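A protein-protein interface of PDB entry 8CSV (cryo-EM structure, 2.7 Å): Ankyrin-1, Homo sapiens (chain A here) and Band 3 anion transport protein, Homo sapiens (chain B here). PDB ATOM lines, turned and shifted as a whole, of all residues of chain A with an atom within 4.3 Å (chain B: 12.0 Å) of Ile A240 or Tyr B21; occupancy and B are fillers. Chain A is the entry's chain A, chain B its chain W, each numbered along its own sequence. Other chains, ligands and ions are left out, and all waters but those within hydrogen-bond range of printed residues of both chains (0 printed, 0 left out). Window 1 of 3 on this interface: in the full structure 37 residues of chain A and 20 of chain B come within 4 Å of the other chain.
Printed residues of chain B that touch a printed residue of chain A: Leu B16, Glu B17, Gln B18, Tyr B21 and Asp B23.
Of the 15 printed residues of chain A, 8 touch a printed residue of chain B.
Printed residues of chain A that touch a printed residue of chain B: Phe A207, Asn A238, Ile A240, His A244, Ile A245, Arg A248, Thr A269 and Leu A273.
Hydrophobic or aromatic side chains of chain A that line the printed part of chain B: Phe A207, Ile A240, Ile A245 and Leu A273.
Among the printed residues, Asp or Glu carboxylates within 4 Å of a Lys or Arg side-chain nitrogen of the other chain: Arg A248 with Glu B17.
A ring nitrogen (NE2) of His A244 lies within hydrogen-bond range of the backbone carbonyl oxygen (O) of Leu A273 (2.7 Å).
The side-chain hydroxyl (OG1) of Thr A241 sits at hydrogen-bond distance from the backbone NH (N) of His A244 (3.3 Å).
The backbone NH of Leu A273 lies within hydrogen-bond range of the side-chain hydroxyl of Thr A269, 3.2 Å away.
A ring nitrogen (NE2) of His A211 sits at hydrogen-bond distance from the backbone carbonyl oxygen (O) of Ile A240 (2.9 Å).
OD1 of Asn A238 is in hydrogen-bond range of N of Ile A240, 3.2 Å away.
Among the printed residues, merely in contact across the chains: Ile A245 with Tyr B21, Phe A207 with Leu B16, Leu A273 with Tyr B21, His A244 with Tyr B21, Thr A269 with Tyr B21, Ile A240 with Tyr B21, Arg A248 with Leu B16, Leu A273 with Asp B23 and Asn A238 with Gln B18.
The guanidinium group (NH1) of Arg A248 is in salt-bridge range of the side-chain carboxylate (OE1) of Glu B17 (3.1 Å).
The guanidinium group (NE) of Arg A248 sits at hydrogen-bond distance from the side-chain hydroxyl (OH) of Tyr B21 (3.5 Å).
Printed residues of chain B within 4 Å of Phe A207: Leu B16.
No residue of chain B comes within 4 Å of Pro A236.
No residue of chain B comes within 4 Å of Gly A239.
No residue of chain B comes within 4 Å of Thr A241.
No residue of chain B comes within 4 Å of Pro A242.
Of chain B, only Tyr B21 (3.6 Å) comes within 4 Å of His A244.
Ile A245 touches just one residue of chain B: Tyr B21.
Of chain B, only Leu B16 (3.7 Å), Glu B17 (3.1 Å) and Tyr B21 (3.5 Å) come within 4 Å of Arg A248.
Of chain B, only Tyr B21 (3.6 Å) comes within 4 Å of Thr A269.
Of chain B, only Tyr B21 (3.5 Å) and Asp B23 (3.8 Å) come within 4 Å of Leu A273.
Printed residues of chain A within 4 Å of Leu B16: Phe A207 (3.5 Å) and Arg A248 (3.7 Å).
Glu B22 touches none of the printed residues of chain A.
The nearest residue of chain B that does not touch Ile A240 is Gln B18 (4.3 Å).
The nearest residue of chain A that does not touch Tyr B21 is Cys A278 (4.1 Å).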
ATOM      1  N   PHE A 207       2.298   6.134 -22.853  1.00  0.00           N
ATOM      2  CA  PHE A 207       1.593   5.732 -21.646  1.00  0.00           C
ATOM      3  C   PHE A 207       1.837   6.716 -20.508  1.00  0.00           C
ATOM      4  O   PHE A 207       2.934   7.258 -20.351  1.00  0.00           O
ATOM      5  CB  PHE A 207       2.018   4.327 -21.214  1.00  0.00           C
ATOM      6  CG  PHE A 207       1.417   3.230 -22.044  1.00  0.00           C
ATOM      7  CD1 PHE A 207       0.151   3.368 -22.587  1.00  0.00           C
ATOM      8  CD2 PHE A 207       2.116   2.063 -22.281  1.00  0.00           C
ATOM      9  CE1 PHE A 207      -0.405   2.358 -23.348  1.00  0.00           C
ATOM     10  CE2 PHE A 207       1.566   1.048 -23.040  1.00  0.00           C
ATOM     11  CZ  PHE A 207       0.305   1.197 -23.575  1.00  0.00           C
ATOM     12  N   HIS A 211      -0.627   4.168 -16.098  1.00  0.00           N
ATOM     13  CA  HIS A 211      -0.443   2.875 -16.753  1.00  0.00           C
ATOM     14  C   HIS A 211       0.654   2.064 -16.072  1.00  0.00           C
ATOM     15  O   HIS A 211       0.500   0.857 -15.852  1.00  0.00           O
ATOM     16  CB  HIS A 211      -0.108   3.073 -18.231  1.00  0.00           C
ATOM     17  CG  HIS A 211      -1.254   3.570 -19.056  1.00  0.00           C
ATOM     18  ND1 HIS A 211      -1.632   4.895 -19.085  1.00  0.00           N
ATOM     19  CD2 HIS A 211      -2.101   2.920 -19.888  1.00  0.00           C
ATOM     20  CE1 HIS A 211      -2.664   5.039 -19.897  1.00  0.00           C
ATOM     21  NE2 HIS A 211      -2.969   3.855 -20.396  1.00  0.00           N
ATOM     22  N   PHE A 234      -7.512   7.288 -19.619  1.00  0.00           N
ATOM     23  CA  PHE A 234      -6.618   7.874 -20.606  1.00  0.00           C
ATOM     24  C   PHE A 234      -6.376   6.845 -21.701  1.00  0.00           C
ATOM     25  O   PHE A 234      -5.807   5.780 -21.442  1.00  0.00           O
ATOM     26  CB  PHE A 234      -5.297   8.316 -19.976  1.00  0.00           C
ATOM     27  CG  PHE A 234      -4.466   9.186 -20.875  1.00  0.00           C
ATOM     28  CD1 PHE A 234      -3.569   8.627 -21.771  1.00  0.00           C
ATOM     29  CD2 PHE A 234      -4.591  10.563 -20.833  1.00  0.00           C
ATOM     30  CE1 PHE A 234      -2.811   9.424 -22.601  1.00  0.00           C
ATOM     31  CE2 PHE A 234      -3.835  11.366 -21.660  1.00  0.00           C
ATOM     32  CZ  PHE A 234      -2.943  10.796 -22.546  1.00  0.00           C
ATOM     33  N   PRO A 236      -4.519   5.945 -25.065  1.00  0.00           N
ATOM     34  CA  PRO A 236      -3.494   6.252 -26.071  1.00  0.00           C
ATOM     35  C   PRO A 236      -3.934   5.857 -27.470  1.00  0.00           C
ATOM     36  O   PRO A 236      -5.096   5.495 -27.686  1.00  0.00           O
ATOM     37  CB  PRO A 236      -2.286   5.424 -25.611  1.00  0.00           C
ATOM     38  CG  PRO A 236      -2.577   5.060 -24.193  1.00  0.00           C
ATOM     39  CD  PRO A 236      -4.058   4.934 -24.105  1.00  0.00           C
ATOM     40  N   ASN A 238      -3.079   3.232 -29.138  1.00  0.00           N
ATOM     41  CA  ASN A 238      -3.363   1.804 -29.184  1.00  0.00           C
ATOM     42  C   ASN A 238      -4.628   1.415 -28.430  1.00  0.00           C
ATOM     43  O   ASN A 238      -5.052   0.258 -28.520  1.00  0.00           O
ATOM     44  CB  ASN A 238      -2.173   1.007 -28.633  1.00  0.00           C
ATOM     45  CG  ASN A 238      -1.722   1.489 -27.265  1.00  0.00           C
ATOM     46  OD1 ASN A 238      -2.415   2.255 -26.599  1.00  0.00           O
ATOM     47  ND2 ASN A 238      -0.550   1.035 -26.840  1.00  0.00           N
ATOM     48  N   GLY A 239      -5.236   2.342 -27.692  1.00  0.00           N
ATOM     49  CA  GLY A 239      -6.470   2.064 -26.988  1.00  0.00           C
ATOM     50  C   GLY A 239      -6.322   1.342 -25.669  1.00  0.00           C
ATOM     51  O   GLY A 239      -7.333   0.921 -25.098  1.00  0.00           O
ATOM     52  N   ILE A 240      -5.104   1.193 -25.159  1.00  0.00           N
ATOM     53  CA  ILE A 240      -4.854   0.422 -23.947  1.00  0.00           C
ATOM     54  C   ILE A 240      -5.028   1.340 -22.741  1.00  0.00           C
ATOM     55  O   ILE A 240      -4.171   2.180 -22.456  1.00  0.00           O
ATOM     56  CB  ILE A 240      -3.459  -0.211 -23.965  1.00  0.00           C
ATOM     57  CG1 ILE A 240      -3.301  -1.113 -25.190  1.00  0.00           C
ATOM     58  CG2 ILE A 240      -3.223  -1.003 -22.697  1.00  0.00           C
ATOM     59  CD1 ILE A 240      -1.924  -1.719 -25.323  1.00  0.00           C
ATOM     60  N   THR A 241      -6.138   1.175 -22.032  1.00  0.00           N
ATOM     61  CA  THR A 241      -6.424   1.933 -20.827  1.00  0.00           C
ATOM     62  C   THR A 241      -5.737   1.298 -19.620  1.00  0.00           C
ATOM     63  O   THR A 241      -5.298   0.148 -19.682  1.00  0.00           O
ATOM     64  CB  THR A 241      -7.933   2.004 -20.607  1.00  0.00           C
ATOM     65  OG1 THR A 241      -8.468   0.679 -20.514  1.00  0.00           O
ATOM     66  CG2 THR A 241      -8.600   2.733 -21.756  1.00  0.00           C
ATOM     67  N   PRO A 242      -5.598   2.042 -18.514  1.00  0.00           N
ATOM     68  CA  PRO A 242      -5.080   1.413 -17.284  1.00  0.00           C
ATOM     69  C   PRO A 242      -5.925   0.244 -16.803  1.00  0.00           C
ATOM     70  O   PRO A 242      -5.385  -0.709 -16.226  1.00  0.00           O
ATOM     71  CB  PRO A 242      -5.080   2.569 -16.278  1.00  0.00           C
ATOM     72  CG  PRO A 242      -4.932   3.782 -17.111  1.00  0.00           C
ATOM     73  CD  PRO A 242      -5.693   3.507 -18.375  1.00  0.00           C
ATOM     74  N   HIS A 244      -7.389  -1.873 -18.794  1.00  0.00           N
ATOM     75  CA  HIS A 244      -6.929  -2.984 -19.623  1.00  0.00           C
ATOM     76  C   HIS A 244      -5.665  -3.611 -19.056  1.00  0.00           C
ATOM     77  O   HIS A 244      -5.554  -4.840 -18.974  1.00  0.00           O
ATOM     78  CB  HIS A 244      -6.669  -2.511 -21.055  1.00  0.00           C
ATOM     79  CG  HIS A 244      -7.902  -2.372 -21.891  1.00  0.00           C
ATOM     80  ND1 HIS A 244      -8.608  -1.193 -21.986  1.00  0.00           N
ATOM     81  CD2 HIS A 244      -8.545  -3.261 -22.684  1.00  0.00           C
ATOM     82  CE1 HIS A 244      -9.639  -1.364 -22.795  1.00  0.00           C
ATOM     83  NE2 HIS A 244      -9.622  -2.609 -23.231  1.00  0.00           N
ATOM     84  N   ILE A 245      -4.700  -2.780 -18.656  1.00  0.00           N
ATOM     85  CA  ILE A 245      -3.440  -3.291 -18.123  1.00  0.00           C
ATOM     86  C   ILE A 245      -3.678  -4.042 -16.820  1.00  0.00           C
ATOM     87  O   ILE A 245      -3.130  -5.127 -16.598  1.00  0.00           O
ATOM     88  CB  ILE A 245      -2.432  -2.144 -17.934  1.00  0.00           C
ATOM     89  CG1 ILE A 245      -2.133  -1.471 -19.272  1.00  0.00           C
ATOM     90  CG2 ILE A 245      -1.156  -2.659 -17.315  1.00  0.00           C
ATOM     91  CD1 ILE A 245      -1.095  -0.382 -19.184  1.00  0.00           C
ATOM     92  N   ARG A 248      -5.321  -7.384 -17.576  1.00  0.00           N
ATOM     93  CA  ARG A 248      -4.401  -8.328 -18.200  1.00  0.00           C
ATOM     94  C   ARG A 248      -3.385  -8.862 -17.198  1.00  0.00           C
ATOM     95  O   ARG A 248      -3.035 -10.046 -17.233  1.00  0.00           O
ATOM     96  CB  ARG A 248      -3.698  -7.655 -19.380  1.00  0.00           C
ATOM     97  CG  ARG A 248      -3.261  -8.592 -20.501  1.00  0.00           C
ATOM     98  CD  ARG A 248      -1.907  -9.231 -20.230  1.00  0.00           C
ATOM     99  NE  ARG A 248      -0.866  -8.237 -20.001  1.00  0.00           N
ATOM    100  CZ  ARG A 248       0.406  -8.525 -19.768  1.00  0.00           C
ATOM    101  NH1 ARG A 248       0.836  -9.775 -19.726  1.00  0.00           N
ATOM    102  NH2 ARG A 248       1.271  -7.533 -19.575  1.00  0.00           N
ATOM    103  N   THR A 269      -9.665  -1.578 -27.396  1.00  0.00           N
ATOM    104  CA  THR A 269      -8.342  -1.221 -27.891  1.00  0.00           C
ATOM    105  C   THR A 269      -8.400  -1.094 -29.414  1.00  0.00           C
ATOM    106  O   THR A 269      -9.471  -1.082 -30.026  1.00  0.00           O
ATOM    107  CB  THR A 269      -7.310  -2.251 -27.442  1.00  0.00           C
ATOM    108  OG1 THR A 269      -7.617  -3.522 -28.026  1.00  0.00           O
ATOM    109  CG2 THR A 269      -7.316  -2.383 -25.933  1.00  0.00           C
ATOM    110  N   LEU A 273     -10.283  -5.217 -28.103  1.00  0.00           N
ATOM    111  CA  LEU A 273     -10.255  -6.066 -26.920  1.00  0.00           C
ATOM    112  C   LEU A 273     -10.766  -5.278 -25.720  1.00  0.00           C
ATOM    113  O   LEU A 273     -10.203  -4.236 -25.369  1.00  0.00           O
ATOM    114  CB  LEU A 273      -8.845  -6.587 -26.650  1.00  0.00           C
ATOM    115  CG  LEU A 273      -8.472  -7.961 -27.209  1.00  0.00           C
ATOM    116  CD1 LEU A 273      -8.241  -7.902 -28.708  1.00  0.00           C
ATOM    117  CD2 LEU A 273      -7.250  -8.508 -26.497  1.00  0.00           C
ATOM    118  N   CYS A 278      -9.082  -9.261 -21.907  1.00  0.00           N
ATOM    119  CA  CYS A 278      -7.747  -9.342 -21.324  1.00  0.00           C
ATOM    120  C   CYS A 278      -7.739 -10.217 -20.078  1.00  0.00           C
ATOM    121  O   CYS A 278      -6.794 -10.981 -19.854  1.00  0.00           O
ATOM    122  CB  CYS A 278      -7.233  -7.939 -20.997  1.00  0.00           C
ATOM    123  SG  CYS A 278      -7.249  -6.788 -22.388  1.00  0.00           S
ATOM    124  N   MET B  12      11.062  -0.596 -20.611  1.00  0.00           N
ATOM    125  CA  MET B  12       9.702  -0.426 -20.108  1.00  0.00           C
ATOM    126  C   MET B  12       8.670  -0.833 -21.153  1.00  0.00           C
ATOM    127  O   MET B  12       7.650  -1.446 -20.818  1.00  0.00           O
ATOM    128  CB  MET B  12       9.478   1.019 -19.665  1.00  0.00           C
ATOM    129  CG  MET B  12       8.087   1.285 -19.112  1.00  0.00           C
ATOM    130  SD  MET B  12       7.629   0.148 -17.788  1.00  0.00           S
ATOM    131  CE  MET B  12       8.839   0.564 -16.536  1.00  0.00           C
ATOM    132  N   GLU B  13       8.916  -0.500 -22.423  1.00  0.00           N
ATOM    133  CA  GLU B  13       8.010  -0.915 -23.490  1.00  0.00           C
ATOM    134  C   GLU B  13       7.973  -2.431 -23.622  1.00  0.00           C
ATOM    135  O   GLU B  13       6.905  -3.018 -23.836  1.00  0.00           O
ATOM    136  CB  GLU B  13       8.427  -0.269 -24.812  1.00  0.00           C
ATOM    137  CG  GLU B  13       7.519  -0.608 -25.983  1.00  0.00           C
ATOM    138  CD  GLU B  13       7.927   0.096 -27.264  1.00  0.00           C
ATOM    139  OE1 GLU B  13       8.921   0.851 -27.238  1.00  0.00           O
ATOM    140  OE2 GLU B  13       7.254  -0.107 -28.296  1.00  0.00           O
ATOM    141  N   GLU B  14       9.132  -3.082 -23.502  1.00  0.00           N
ATOM    142  CA  GLU B  14       9.168  -4.541 -23.532  1.00  0.00           C
ATOM    143  C   GLU B  14       8.432  -5.139 -22.338  1.00  0.00           C
ATOM    144  O   GLU B  14       7.755  -6.166 -22.467  1.00  0.00           O
ATOM    145  CB  GLU B  14      10.616  -5.029 -23.572  1.00  0.00           C
ATOM    146  CG  GLU B  14      11.342  -4.733 -24.875  1.00  0.00           C
ATOM    147  CD  GLU B  14      10.890  -5.628 -26.015  1.00  0.00           C
ATOM    148  OE1 GLU B  14      10.333  -6.713 -25.742  1.00  0.00           O
ATOM    149  OE2 GLU B  14      11.091  -5.245 -27.188  1.00  0.00           O
ATOM    150  N   ASN B  15       8.564  -4.518 -21.164  1.00  0.00           N
ATOM    151  CA  ASN B  15       7.896  -5.029 -19.970  1.00  0.00           C
ATOM    152  C   ASN B  15       6.383  -4.866 -20.058  1.00  0.00           C
ATOM    153  O   ASN B  15       5.634  -5.739 -19.605  1.00  0.00           O
ATOM    154  CB  ASN B  15       8.434  -4.325 -18.726  1.00  0.00           C
ATOM    155  CG  ASN B  15       9.863  -4.712 -18.409  1.00  0.00           C
ATOM    156  OD1 ASN B  15      10.283  -5.840 -18.663  1.00  0.00           O
ATOM    157  ND2 ASN B  15      10.620  -3.774 -17.852  1.00  0.00           N
ATOM    158  N   LEU B  16       5.915  -3.754 -20.631  1.00  0.00           N
ATOM    159  CA  LEU B  16       4.480  -3.495 -20.680  1.00  0.00           C
ATOM    160  C   LEU B  16       3.757  -4.451 -21.621  1.00  0.00           C
ATOM    161  O   LEU B  16       2.547  -4.655 -21.476  1.00  0.00           O
ATOM    162  CB  LEU B  16       4.224  -2.043 -21.082  1.00  0.00           C
ATOM    163  CG  LEU B  16       4.545  -1.024 -19.985  1.00  0.00           C
ATOM    164  CD1 LEU B  16       4.670   0.374 -20.560  1.00  0.00           C
ATOM    165  CD2 LEU B  16       3.494  -1.065 -18.887  1.00  0.00           C
ATOM    166  N   GLU B  17       4.477  -5.035 -22.583  1.00  0.00           N
ATOM    167  CA  GLU B  17       3.963  -6.097 -23.452  1.00  0.00           C
ATOM    168  C   GLU B  17       2.719  -5.644 -24.221  1.00  0.00           C
ATOM    169  O   GLU B  17       1.616  -6.163 -24.039  1.00  0.00           O
ATOM    170  CB  GLU B  17       3.685  -7.373 -22.649  1.00  0.00           C
ATOM    171  CG  GLU B  17       4.912  -7.956 -21.969  1.00  0.00           C
ATOM    172  CD  GLU B  17       4.608  -9.225 -21.196  1.00  0.00           C
ATOM    173  OE1 GLU B  17       3.468  -9.724 -21.295  1.00  0.00           O
ATOM    174  OE2 GLU B  17       5.508  -9.721 -20.488  1.00  0.00           O
ATOM    175  N   GLN B  18       2.920  -4.651 -25.090  1.00  0.00           N
ATOM    176  CA  GLN B  18       1.820  -4.124 -25.891  1.00  0.00           C
ATOM    177  C   GLN B  18       1.244  -5.163 -26.845  1.00  0.00           C
ATOM    178  O   GLN B  18       0.093  -5.024 -27.274  1.00  0.00           O
ATOM    179  CB  GLN B  18       2.287  -2.900 -26.683  1.00  0.00           C
ATOM    180  CG  GLN B  18       2.980  -1.843 -25.842  1.00  0.00           C
ATOM    181  CD  GLN B  18       3.440  -0.653 -26.664  1.00  0.00           C
ATOM    182  OE1 GLN B  18       4.257   0.149 -26.212  1.00  0.00           O
ATOM    183  NE2 GLN B  18       2.914  -0.531 -27.877  1.00  0.00           N
ATOM    184  N   GLU B  19       2.014  -6.200 -27.186  1.00  0.00           N
ATOM    185  CA  GLU B  19       1.514  -7.235 -28.083  1.00  0.00           C
ATOM    186  C   GLU B  19       0.456  -8.103 -27.414  1.00  0.00           C
ATOM    187  O   GLU B  19      -0.381  -8.698 -28.103  1.00  0.00           O
ATOM    188  CB  GLU B  19       2.671  -8.101 -28.580  1.00  0.00           C
ATOM    189  N   GLU B  20       0.473  -8.189 -26.082  1.00  0.00           N
ATOM    190  CA  GLU B  20      -0.483  -9.022 -25.360  1.00  0.00           C
ATOM    191  C   GLU B  20      -1.895  -8.453 -25.365  1.00  0.00           C
ATOM    192  O   GLU B  20      -2.823  -9.146 -24.934  1.00  0.00           O
ATOM    193  CB  GLU B  20      -0.014  -9.226 -23.917  1.00  0.00           C
ATOM    194  CG  GLU B  20       1.304  -9.975 -23.788  1.00  0.00           C
ATOM    195  CD  GLU B  20       1.199 -11.433 -24.198  1.00  0.00           C
ATOM    196  OE1 GLU B  20       0.083 -11.993 -24.141  1.00  0.00           O
ATOM    197  OE2 GLU B  20       2.233 -12.020 -24.578  1.00  0.00           O
ATOM    198  N   TYR B  21      -2.081  -7.220 -25.828  1.00  0.00           N
ATOM    199  CA  TYR B  21      -3.390  -6.586 -25.881  1.00  0.00           C
ATOM    200  C   TYR B  21      -3.991  -6.608 -27.280  1.00  0.00           C
ATOM    201  O   TYR B  21      -5.018  -5.962 -27.513  1.00  0.00           O
ATOM    202  CB  TYR B  21      -3.297  -5.147 -25.368  1.00  0.00           C
ATOM    203  CG  TYR B  21      -2.764  -5.049 -23.957  1.00  0.00           C
ATOM    204  CD1 TYR B  21      -3.626  -5.039 -22.869  1.00  0.00           C
ATOM    205  CD2 TYR B  21      -1.399  -4.976 -23.713  1.00  0.00           C
ATOM    206  CE1 TYR B  21      -3.142  -4.954 -21.579  1.00  0.00           C
ATOM    207  CE2 TYR B  21      -0.908  -4.895 -22.427  1.00  0.00           C
ATOM    208  CZ  TYR B  21      -1.783  -4.884 -21.365  1.00  0.00           C
ATOM    209  OH  TYR B  21      -1.292  -4.800 -20.083  1.00  0.00           O
ATOM    210  N   GLU B  22      -3.380  -7.335 -28.208  1.00  0.00           N
ATOM    211  CA  GLU B  22      -3.845  -7.418 -29.583  1.00  0.00           C
ATOM    212  C   GLU B  22      -4.326  -8.830 -29.889  1.00  0.00           C
ATOM    213  O   GLU B  22      -3.894  -9.801 -29.261  1.00  0.00           O
ATOM    214  CB  GLU B  22      -2.735  -7.033 -30.565  1.00  0.00           C
ATOM    215  CG  GLU B  22      -2.002  -5.755 -30.211  1.00  0.00           C
ATOM    216  CD  GLU B  22      -0.874  -5.448 -31.176  1.00  0.00           C
ATOM    217  OE1 GLU B  22      -0.812  -6.091 -32.245  1.00  0.00           O
ATOM    218  OE2 GLU B  22      -0.047  -4.566 -30.864  1.00  0.00           O
ATOM    219  N   ASP B  23      -5.231  -8.935 -30.861  1.00  0.00           N
ATOM    220  CA  ASP B  23      -5.657 -10.233 -31.362  1.00  0.00           C
ATOM    221  C   ASP B  23      -4.691 -10.639 -32.465  1.00  0.00           C
ATOM    222  O   ASP B  23      -4.659  -9.981 -33.517  1.00  0.00           O
ATOM    223  CB  ASP B  23      -7.084 -10.167 -31.890  1.00  0.00           C
ATOM    224  CG  ASP B  23      -7.732 -11.537 -32.009  1.00  0.00           C
ATOM    225  OD1 ASP B  23      -7.011 -12.534 -32.218  1.00  0.00           O
ATOM    226  OD2 ASP B  23      -8.973 -11.615 -31.892  1.00  0.00           O
ATOM    227  N   PRO B  24      -3.884 -11.689 -32.277  1.00  0.00           N
ATOM    228  CA  PRO B  24      -2.852 -12.002 -33.285  1.00  0.00           C
ATOM    229  C   PRO B  24      -3.420 -12.406 -34.634  1.00  0.00           C
ATOM    230  O   PRO B  24      -3.131 -11.752 -35.646  1.00  0.00           O
ATOM    231  CB  PRO B  24      -2.064 -13.146 -32.627  1.00  0.00           C
ATOM    232  CG  PRO B  24      -2.390 -13.063 -31.165  1.00  0.00           C
ATOM    233  CD  PRO B  24      -3.801 -12.572 -31.105  1.00  0.00           C
ATOM    234  N   ASP B  25      -4.241 -13.453 -34.672  1.00  0.00           N
ATOM    235  CA  ASP B  25      -4.809 -13.973 -35.908  1.00  0.00           C
ATOM    236  C   ASP B  25      -5.835 -15.038 -35.555  1.00  0.00           C
ATOM    237  O   ASP B  25      -5.971 -15.433 -34.393  1.00  0.00           O
ATOM    238  CB  ASP B  25      -3.733 -14.560 -36.832  1.00  0.00           C
